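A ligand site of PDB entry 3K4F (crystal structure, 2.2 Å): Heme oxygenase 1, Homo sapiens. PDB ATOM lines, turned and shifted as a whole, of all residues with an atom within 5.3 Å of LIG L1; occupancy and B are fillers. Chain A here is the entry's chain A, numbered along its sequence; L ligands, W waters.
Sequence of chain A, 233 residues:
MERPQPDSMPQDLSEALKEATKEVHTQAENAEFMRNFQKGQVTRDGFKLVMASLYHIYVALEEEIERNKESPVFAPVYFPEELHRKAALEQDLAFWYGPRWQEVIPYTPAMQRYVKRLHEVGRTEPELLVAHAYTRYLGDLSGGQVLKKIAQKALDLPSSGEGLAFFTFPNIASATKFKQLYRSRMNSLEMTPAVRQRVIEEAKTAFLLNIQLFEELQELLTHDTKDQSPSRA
Residues that only touch LIG L1: Ala 28, Glu 29, Met 34, Gln 38, Thr 135, Leu 138, Gly 139, Ser 142, Phe 207 and Asn 210. Of the 20 residues printed, 15 come within 4 Å of LIG L1. The nearest printed residue that does not touch LIG L1 is Arg 136 (4.2 Å).
The side-chain hydroxyl (OH) of Tyr 134 lies within hydrogen-bond range of an oxygen (O3) of LIG L1, 2.8 Å away. O1 of LIG L1 is in salt-bridge range of NZ of Lys 179, at 3.9 Å. NE2 of His 25 is bound to FE1 of LIG L1 (2.2 Å). The side-chain amino group of Lys 18 lies within salt-bridge range of an oxygen (O2) of LIG L1. The guanidinium group of Arg 183 is in salt-bridge range of an oxygen (O4) of LIG L1, 2.6 Å away.
The side-chain amide nitrogen (ND2) of Asn 210 is in hydrogen-bond range of the backbone carbonyl oxygen (O) of Ala 206, 2.7 Å away. The side-chain hydroxyl (OG) of Ser 142 sits at hydrogen-bond distance from the side-chain amino group (NZ) of Lys 179, 2.8 Å away. OD1 of Asn 210 sits at hydrogen-bond distance from NH1 of Arg 136, at 2.8 Å. ND2 of Asn 210 lies within hydrogen-bond range of OH of Tyr 114. O of Leu 138 lies within hydrogen-bond range of OG of Ser 142 (2.7 Å). A ring nitrogen (ND1) of His 25 lies within hydrogen-bond range of the side-chain carboxylate of Glu 29, 3.2 Å away.
FE1 of LIG L1 is bound by N3 of LG2 L2 (2.3 Å).
Water W2 lies within hydrogen-bond range of O3 of LIG L1 (2.7 Å), O of Ser 14 (2.9 Å) and NE of Arg 183 (3.4 Å). Water W3 bridges NH2 of Arg 136 and O1 of LG2 L2. Water W4 bridges O of Thr 135 (2.8 Å) and NH2 of Arg 136 (3.2 Å).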
ATOM      1  N   SER A  14      -9.462 -21.444 -32.481  1.00  0.00           N
ATOM      2  CA  SER A  14      -9.044 -22.065 -31.229  1.00  0.00           C
ATOM      3  C   SER A  14      -7.516 -22.104 -31.077  1.00  0.00           C
ATOM      4  O   SER A  14      -6.986 -21.802 -30.012  1.00  0.00           O
ATOM      5  CB  SER A  14      -9.622 -23.473 -31.099  1.00  0.00           C
ATOM      6  OG  SER A  14      -9.153 -24.328 -32.120  1.00  0.00           O
ATOM      7  N   LYS A  18      -5.025 -19.575 -28.704  1.00  0.00           N
ATOM      8  CA  LYS A  18      -4.024 -20.210 -27.847  1.00  0.00           C
ATOM      9  C   LYS A  18      -2.629 -19.641 -28.098  1.00  0.00           C
ATOM     10  O   LYS A  18      -1.893 -19.361 -27.146  1.00  0.00           O
ATOM     11  CB  LYS A  18      -4.049 -21.733 -28.051  1.00  0.00           C
ATOM     12  CG  LYS A  18      -3.349 -22.523 -26.947  1.00  0.00           C
ATOM     13  CD  LYS A  18      -3.659 -23.999 -27.049  1.00  0.00           C
ATOM     14  CE  LYS A  18      -3.219 -24.741 -25.794  1.00  0.00           C
ATOM     15  NZ  LYS A  18      -3.544 -26.192 -25.873  1.00  0.00           N
ATOM     16  N   HIS A  25      -0.600 -15.683 -20.732  1.00  0.00           N
ATOM     17  CA  HIS A  25      -0.901 -16.829 -19.882  1.00  0.00           C
ATOM     18  C   HIS A  25       0.277 -17.144 -18.959  1.00  0.00           C
ATOM     19  O   HIS A  25       0.074 -17.501 -17.790  1.00  0.00           O
ATOM     20  CB  HIS A  25      -1.265 -18.048 -20.725  1.00  0.00           C
ATOM     21  CG  HIS A  25      -1.856 -19.176 -19.944  1.00  0.00           C
ATOM     22  ND1 HIS A  25      -1.187 -20.365 -19.732  1.00  0.00           N
ATOM     23  CD2 HIS A  25      -3.041 -19.296 -19.307  1.00  0.00           C
ATOM     24  CE1 HIS A  25      -1.946 -21.175 -19.015  1.00  0.00           C
ATOM     25  NE2 HIS A  25      -3.080 -20.550 -18.746  1.00  0.00           N
ATOM     26  N   ALA A  28       0.265 -14.709 -16.147  1.00  0.00           N
ATOM     27  CA  ALA A  28      -0.698 -15.146 -15.140  1.00  0.00           C
ATOM     28  C   ALA A  28      -0.111 -16.213 -14.230  1.00  0.00           C
ATOM     29  O   ALA A  28      -0.323 -16.187 -13.018  1.00  0.00           O
ATOM     30  CB  ALA A  28      -1.970 -15.643 -15.806  1.00  0.00           C
ATOM     31  N   GLU A  29       0.637 -17.145 -14.824  1.00  0.00           N
ATOM     32  CA  GLU A  29       1.347 -18.187 -14.078  1.00  0.00           C
ATOM     33  C   GLU A  29       2.370 -17.600 -13.116  1.00  0.00           C
ATOM     34  O   GLU A  29       2.567 -18.106 -12.008  1.00  0.00           O
ATOM     35  CB  GLU A  29       2.043 -19.164 -15.041  1.00  0.00           C
ATOM     36  CG  GLU A  29       1.096 -19.963 -15.940  1.00  0.00           C
ATOM     37  CD  GLU A  29       1.829 -20.877 -16.910  1.00  0.00           C
ATOM     38  OE1 GLU A  29       1.496 -20.847 -18.112  1.00  0.00           O
ATOM     39  OE2 GLU A  29       2.734 -21.616 -16.473  1.00  0.00           O
ATOM     40  N   MET A  34      -1.006 -16.090  -7.773  1.00  0.00           N
ATOM     41  CA  MET A  34      -1.011 -17.398  -8.408  1.00  0.00           C
ATOM     42  C   MET A  34       0.128 -18.280  -7.930  1.00  0.00           C
ATOM     43  O   MET A  34      -0.050 -19.484  -7.747  1.00  0.00           O
ATOM     44  CB  MET A  34      -1.006 -17.248  -9.928  1.00  0.00           C
ATOM     45  CG  MET A  34      -2.198 -16.482 -10.481  1.00  0.00           C
ATOM     46  SD  MET A  34      -3.748 -17.404 -10.501  1.00  0.00           S
ATOM     47  CE  MET A  34      -4.147 -17.561  -8.766  1.00  0.00           C
ATOM     48  N   GLN A  38      -0.808 -21.673  -5.692  1.00  0.00           N
ATOM     49  CA  GLN A  38      -0.294 -22.958  -6.185  1.00  0.00           C
ATOM     50  C   GLN A  38       0.518 -23.699  -5.120  1.00  0.00           C
ATOM     51  O   GLN A  38       0.689 -24.914  -5.184  1.00  0.00           O
ATOM     52  CB  GLN A  38       0.529 -22.750  -7.449  1.00  0.00           C
ATOM     53  CG  GLN A  38       0.486 -23.900  -8.438  1.00  0.00           C
ATOM     54  CD  GLN A  38       0.653 -23.447  -9.889  1.00  0.00           C
ATOM     55  OE1 GLN A  38       0.781 -24.268 -10.790  1.00  0.00           O
ATOM     56  NE2 GLN A  38       0.637 -22.130 -10.104  1.00  0.00           N
ATOM     57  N   TYR A 114     -13.111  -4.991 -15.304  1.00  0.00           N
ATOM     58  CA  TYR A 114     -13.424  -6.246 -15.977  1.00  0.00           C
ATOM     59  C   TYR A 114     -14.900  -6.303 -16.357  1.00  0.00           C
ATOM     60  O   TYR A 114     -15.242  -6.569 -17.508  1.00  0.00           O
ATOM     61  CB  TYR A 114     -13.061  -7.427 -15.063  1.00  0.00           C
ATOM     62  CG  TYR A 114     -12.828  -8.772 -15.749  1.00  0.00           C
ATOM     63  CD1 TYR A 114     -13.546  -9.143 -16.891  1.00  0.00           C
ATOM     64  CD2 TYR A 114     -11.908  -9.680 -15.225  1.00  0.00           C
ATOM     65  CE1 TYR A 114     -13.341 -10.380 -17.502  1.00  0.00           C
ATOM     66  CE2 TYR A 114     -11.706 -10.919 -15.822  1.00  0.00           C
ATOM     67  CZ  TYR A 114     -12.420 -11.261 -16.952  1.00  0.00           C
ATOM     68  OH  TYR A 114     -12.210 -12.482 -17.545  1.00  0.00           O
ATOM     69  N   TYR A 134     -14.329 -17.760 -23.941  1.00  0.00           N
ATOM     70  CA  TYR A 134     -13.179 -18.656 -24.056  1.00  0.00           C
ATOM     71  C   TYR A 134     -12.252 -18.512 -22.845  1.00  0.00           C
ATOM     72  O   TYR A 134     -11.861 -19.498 -22.232  1.00  0.00           O
ATOM     73  CB  TYR A 134     -12.400 -18.366 -25.354  1.00  0.00           C
ATOM     74  CG  TYR A 134     -10.995 -18.918 -25.364  1.00  0.00           C
ATOM     75  CD1 TYR A 134     -10.759 -20.278 -25.560  1.00  0.00           C
ATOM     76  CD2 TYR A 134      -9.898 -18.078 -25.180  1.00  0.00           C
ATOM     77  CE1 TYR A 134      -9.458 -20.785 -25.568  1.00  0.00           C
ATOM     78  CE2 TYR A 134      -8.599 -18.572 -25.193  1.00  0.00           C
ATOM     79  CZ  TYR A 134      -8.387 -19.933 -25.386  1.00  0.00           C
ATOM     80  OH  TYR A 134      -7.105 -20.430 -25.403  1.00  0.00           O
ATOM     81  N   THR A 135     -11.904 -17.264 -22.529  1.00  0.00           N
ATOM     82  CA  THR A 135     -10.958 -16.943 -21.464  1.00  0.00           C
ATOM     83  C   THR A 135     -11.461 -17.399 -20.099  1.00  0.00           C
ATOM     84  O   THR A 135     -10.706 -17.991 -19.314  1.00  0.00           O
ATOM     85  CB  THR A 135     -10.645 -15.415 -21.456  1.00  0.00           C
ATOM     86  OG1 THR A 135     -10.240 -15.006 -22.765  1.00  0.00           O
ATOM     87  CG2 THR A 135      -9.540 -15.090 -20.473  1.00  0.00           C
ATOM     88  N   ARG A 136     -12.740 -17.158 -19.820  1.00  0.00           N
ATOM     89  CA  ARG A 136     -13.357 -17.565 -18.561  1.00  0.00           C
ATOM     90  C   ARG A 136     -13.618 -19.064 -18.498  1.00  0.00           C
ATOM     91  O   ARG A 136     -13.003 -19.767 -17.687  1.00  0.00           O
ATOM     92  CB  ARG A 136     -14.647 -16.785 -18.290  1.00  0.00           C
ATOM     93  CG  ARG A 136     -14.433 -15.449 -17.588  1.00  0.00           C
ATOM     94  CD  ARG A 136     -14.542 -15.567 -16.059  1.00  0.00           C
ATOM     95  NE  ARG A 136     -13.514 -16.425 -15.466  1.00  0.00           N
ATOM     96  CZ  ARG A 136     -12.300 -16.007 -15.102  1.00  0.00           C
ATOM     97  NH1 ARG A 136     -11.942 -14.749 -15.276  1.00  0.00           N
ATOM     98  NH2 ARG A 136     -11.446 -16.868 -14.561  1.00  0.00           N
ATOM     99  N   LEU A 138     -13.178 -21.963 -20.511  1.00  0.00           N
ATOM    100  CA  LEU A 138     -12.162 -22.987 -20.797  1.00  0.00           C
ATOM    101  C   LEU A 138     -11.007 -22.976 -19.797  1.00  0.00           C
ATOM    102  O   LEU A 138     -10.459 -24.025 -19.470  1.00  0.00           O
ATOM    103  CB  LEU A 138     -11.659 -22.892 -22.240  1.00  0.00           C
ATOM    104  CG  LEU A 138     -12.301 -23.868 -23.242  1.00  0.00           C
ATOM    105  CD1 LEU A 138     -13.833 -23.873 -23.176  1.00  0.00           C
ATOM    106  CD2 LEU A 138     -11.815 -23.616 -24.659  1.00  0.00           C
ATOM    107  N   GLY A 139     -10.662 -21.782 -19.322  1.00  0.00           N
ATOM    108  CA  GLY A 139      -9.690 -21.640 -18.248  1.00  0.00           C
ATOM    109  C   GLY A 139     -10.176 -22.246 -16.944  1.00  0.00           C
ATOM    110  O   GLY A 139      -9.506 -23.084 -16.344  1.00  0.00           O
ATOM    111  N   SER A 142     -10.486 -26.041 -17.158  1.00  0.00           N
ATOM    112  CA  SER A 142      -9.183 -26.708 -17.144  1.00  0.00           C
ATOM    113  C   SER A 142      -8.583 -26.828 -15.749  1.00  0.00           C
ATOM    114  O   SER A 142      -8.036 -27.872 -15.393  1.00  0.00           O
ATOM    115  CB  SER A 142      -8.194 -25.969 -18.056  1.00  0.00           C
ATOM    116  OG  SER A 142      -8.635 -25.952 -19.402  1.00  0.00           O
ATOM    117  N   LYS A 179     -14.153 -29.538 -24.189  1.00  0.00           N
ATOM    118  CA  LYS A 179     -13.227 -28.546 -24.744  1.00  0.00           C
ATOM    119  C   LYS A 179     -13.010 -28.715 -26.242  1.00  0.00           C
ATOM    120  O   LYS A 179     -12.936 -27.730 -26.964  1.00  0.00           O
ATOM    121  CB  LYS A 179     -11.884 -28.542 -23.995  1.00  0.00           C
ATOM    122  CG  LYS A 179     -11.915 -27.798 -22.661  1.00  0.00           C
ATOM    123  CD  LYS A 179     -10.516 -27.427 -22.186  1.00  0.00           C
ATOM    124  CE  LYS A 179      -9.856 -28.553 -21.409  1.00  0.00           C
ATOM    125  NZ  LYS A 179      -8.439 -28.228 -21.075  1.00  0.00           N
ATOM    126  N   ARG A 183     -14.049 -25.853 -28.851  1.00  0.00           N
ATOM    127  CA  ARG A 183     -13.063 -25.377 -29.828  1.00  0.00           C
ATOM    128  C   ARG A 183     -13.612 -25.441 -31.246  1.00  0.00           C
ATOM    129  O   ARG A 183     -13.453 -24.491 -32.031  1.00  0.00           O
ATOM    130  CB  ARG A 183     -11.769 -26.180 -29.732  1.00  0.00           C
ATOM    131  CG  ARG A 183     -10.891 -25.796 -28.562  1.00  0.00           C
ATOM    132  CD  ARG A 183      -9.910 -26.901 -28.285  1.00  0.00           C
ATOM    133  NE  ARG A 183      -9.164 -26.685 -27.044  1.00  0.00           N
ATOM    134  CZ  ARG A 183      -8.690 -27.660 -26.286  1.00  0.00           C
ATOM    135  NH1 ARG A 183      -8.890 -28.926 -26.608  1.00  0.00           N
ATOM    136  NH2 ARG A 183      -8.018 -27.362 -25.176  1.00  0.00           N
ATOM    137  N   ALA A 206      -8.675  -9.734 -22.296  1.00  0.00           N
ATOM    138  CA  ALA A 206      -9.320 -10.547 -21.264  1.00  0.00           C
ATOM    139  C   ALA A 206      -8.323 -11.142 -20.279  1.00  0.00           C
ATOM    140  O   ALA A 206      -8.534 -11.095 -19.057  1.00  0.00           O
ATOM    141  CB  ALA A 206     -10.159 -11.648 -21.904  1.00  0.00           C
ATOM    142  N   PHE A 207      -7.219 -11.688 -20.803  1.00  0.00           N
ATOM    143  CA  PHE A 207      -6.123 -12.190 -19.984  1.00  0.00           C
ATOM    144  C   PHE A 207      -5.487 -11.077 -19.146  1.00  0.00           C
ATOM    145  O   PHE A 207      -5.133 -11.295 -17.987  1.00  0.00           O
ATOM    146  CB  PHE A 207      -5.054 -12.846 -20.869  1.00  0.00           C
ATOM    147  CG  PHE A 207      -5.267 -14.312 -21.112  1.00  0.00           C
ATOM    148  CD1 PHE A 207      -4.500 -15.263 -20.438  1.00  0.00           C
ATOM    149  CD2 PHE A 207      -6.221 -14.751 -22.020  1.00  0.00           C
ATOM    150  CE1 PHE A 207      -4.684 -16.611 -20.667  1.00  0.00           C
ATOM    151  CE2 PHE A 207      -6.417 -16.107 -22.245  1.00  0.00           C
ATOM    152  CZ  PHE A 207      -5.651 -17.045 -21.577  1.00  0.00           C
ATOM    153  N   ASN A 210      -7.581 -10.117 -16.215  1.00  0.00           N
ATOM    154  CA  ASN A 210      -7.368 -11.116 -15.172  1.00  0.00           C
ATOM    155  C   ASN A 210      -6.056 -10.888 -14.419  1.00  0.00           C
ATOM    156  O   ASN A 210      -6.017 -10.994 -13.197  1.00  0.00           O
ATOM    157  CB  ASN A 210      -7.411 -12.529 -15.755  1.00  0.00           C
ATOM    158  CG  ASN A 210      -8.825 -13.026 -15.968  1.00  0.00           C
ATOM    159  OD1 ASN A 210      -9.462 -13.520 -15.043  1.00  0.00           O
ATOM    160  ND2 ASN A 210      -9.331 -12.883 -17.192  1.00  0.00           N
ATOM    161  N   PHE A 214      -5.750  -9.943 -10.346  1.00  0.00           N
ATOM    162  CA  PHE A 214      -4.984 -10.682  -9.354  1.00  0.00           C
ATOM    163  C   PHE A 214      -3.817  -9.903  -8.761  1.00  0.00           C
ATOM    164  O   PHE A 214      -3.371 -10.186  -7.646  1.00  0.00           O
ATOM    165  CB  PHE A 214      -4.534 -12.051  -9.898  1.00  0.00           C
ATOM    166  CG  PHE A 214      -5.604 -13.090  -9.874  1.00  0.00           C
ATOM    167  CD1 PHE A 214      -5.803 -13.874  -8.740  1.00  0.00           C
ATOM    168  CD2 PHE A 214      -6.449 -13.283 -10.969  1.00  0.00           C
ATOM    169  CE1 PHE A 214      -6.813 -14.832  -8.702  1.00  0.00           C
ATOM    170  CE2 PHE A 214      -7.457 -14.238 -10.944  1.00  0.00           C
ATOM    171  CZ  PHE A 214      -7.639 -15.019  -9.808  1.00  0.00           C
HETATM  172  C1  LIG L   1      -5.857 -23.648 -19.565  1.00  0.00           C
HETATM  173  C2  LIG L   1      -2.376 -23.240 -16.214  1.00  0.00           C
HETATM  174  C3  LIG L   1      -4.031 -18.810 -15.074  1.00  0.00           C
HETATM  175  C4  LIG L   1      -6.821 -18.877 -19.044  1.00  0.00           C
HETATM  176  C5  LIG L   1      -4.812 -23.966 -18.723  1.00  0.00           C
HETATM  177  C6  LIG L   1      -4.135 -25.248 -18.616  1.00  0.00           C
HETATM  178  C7  LIG L   1      -3.176 -25.136 -17.693  1.00  0.00           C
HETATM  179  C8  LIG L   1      -3.204 -23.777 -17.180  1.00  0.00           C
HETATM  180  C9  LIG L   1      -2.200 -26.244 -17.230  1.00  0.00           C
HETATM  181  C10 LIG L   1      -4.489 -26.523 -19.428  1.00  0.00           C
HETATM  182  C11 LIG L   1      -3.635 -26.574 -20.687  1.00  0.00           C
HETATM  183  C12 LIG L   1      -4.505 -26.960 -21.864  1.00  0.00           C
HETATM  184  O1  LIG L   1      -4.660 -28.183 -22.114  1.00  0.00           O
HETATM  185  O2  LIG L   1      -5.025 -26.036 -22.550  1.00  0.00           O
HETATM  186  C13 LIG L   1      -2.546 -22.024 -15.571  1.00  0.00           C
HETATM  187  C14 LIG L   1      -1.821 -21.562 -14.401  1.00  0.00           C
HETATM  188  C15 LIG L   1      -2.288 -20.338 -14.089  1.00  0.00           C
HETATM  189  C16 LIG L   1      -3.308 -19.993 -15.055  1.00  0.00           C
HETATM  190  C17 LIG L   1      -0.724 -22.371 -13.660  1.00  0.00           C
HETATM  191  C18 LIG L   1      -1.853 -19.417 -12.921  1.00  0.00           C
HETATM  192  C19 LIG L   1      -1.333 -19.912 -11.793  1.00  0.00           C
HETATM  193  C20 LIG L   1      -4.924 -18.415 -16.062  1.00  0.00           C
HETATM  194  C21 LIG L   1      -5.615 -17.143 -16.150  1.00  0.00           C
HETATM  195  C22 LIG L   1      -6.377 -17.171 -17.246  1.00  0.00           C
HETATM  196  C23 LIG L   1      -6.199 -18.456 -17.890  1.00  0.00           C
HETATM  197  C24 LIG L   1      -5.497 -15.962 -15.145  1.00  0.00           C
HETATM  198  C25 LIG L   1      -7.306 -16.040 -17.756  1.00  0.00           C
HETATM  199  C26 LIG L   1      -8.618 -16.127 -17.541  1.00  0.00           C
HETATM  200  C27 LIG L   1      -6.829 -20.149 -19.580  1.00  0.00           C
HETATM  201  C28 LIG L   1      -7.531 -20.549 -20.773  1.00  0.00           C
HETATM  202  C29 LIG L   1      -7.234 -22.042 -20.934  1.00  0.00           C
HETATM  203  C30 LIG L   1      -6.374 -22.393 -19.822  1.00  0.00           C
HETATM  204  C31 LIG L   1      -8.396 -19.668 -21.705  1.00  0.00           C
HETATM  205  C32 LIG L   1      -7.730 -22.967 -22.062  1.00  0.00           C
HETATM  206  C33 LIG L   1      -6.660 -22.982 -23.149  1.00  0.00           C
HETATM  207  C34 LIG L   1      -7.130 -23.795 -24.331  1.00  0.00           C
HETATM  208  O3  LIG L   1      -7.325 -23.215 -25.428  1.00  0.00           O
HETATM  209  O4  LIG L   1      -7.314 -25.036 -24.176  1.00  0.00           O
HETATM  210  N1  LIG L   1      -4.211 -23.092 -17.836  1.00  0.00           N
HETATM  211  N2  LIG L   1      -3.439 -21.038 -15.942  1.00  0.00           N
HETATM  212  N3  LIG L   1      -5.310 -19.188 -17.137  1.00  0.00           N
HETATM  213  N4  LIG L   1      -6.166 -21.258 -19.047  1.00  0.00           N
HETATM  214 FE1  LIG L   1      -4.793 -21.135 -17.495  1.00  0.00          FE
HETATM  215  C1  LG2 L   2      -8.508 -19.876 -12.743  1.00  0.00           C
HETATM  216  N1  LG2 L   2      -7.805 -21.455 -14.503  1.00  0.00           N
HETATM  217  O1  LG2 L   2      -7.327 -19.597 -12.599  1.00  0.00           O
HETATM  218  C2  LG2 L   2      -8.910 -21.008 -13.660  1.00  0.00           C
HETATM  219  C3  LG2 L   2      -7.330 -19.162  -7.888  1.00  0.00           C
HETATM  220  C4  LG2 L   2      -8.395 -19.658  -7.130  1.00  0.00           C
HETATM  221  C5  LG2 L   2      -9.686 -19.653  -7.659  1.00  0.00           C
HETATM  222  C6  LG2 L   2      -9.913 -19.132  -8.936  1.00  0.00           C
HETATM  223  C7  LG2 L   2      -8.855 -18.634  -9.688  1.00  0.00           C
HETATM  224  C8  LG2 L   2      -7.560 -18.650  -9.167  1.00  0.00           C
HETATM  225  C9  LG2 L   2      -9.081 -18.068 -11.075  1.00  0.00           C
HETATM  226  C10 LG2 L   2      -9.614 -19.136 -12.027  1.00  0.00           C
HETATM  227  N2  LG2 L   2      -7.100 -22.570 -14.029  1.00  0.00           N
HETATM  228  C11 LG2 L   2      -6.149 -22.797 -14.969  1.00  0.00           C
HETATM  229  N3  LG2 L   2      -6.294 -21.873 -15.954  1.00  0.00           N
HETATM  230  C12 LG2 L   2      -7.312 -21.038 -15.658  1.00  0.00           C
HETATM  231  O   HOH W   1      -1.627 -23.937 -21.428  1.00  0.00           O
HETATM  232  O   HOH W   2      -7.933 -23.679 -27.997  1.00  0.00           O
HETATM  233  O   HOH W   3      -8.529 -17.520 -14.836  1.00  0.00           O
HETATM  234  O   HOH W   4     -10.123 -18.796 -16.676  1.00  0.00           O
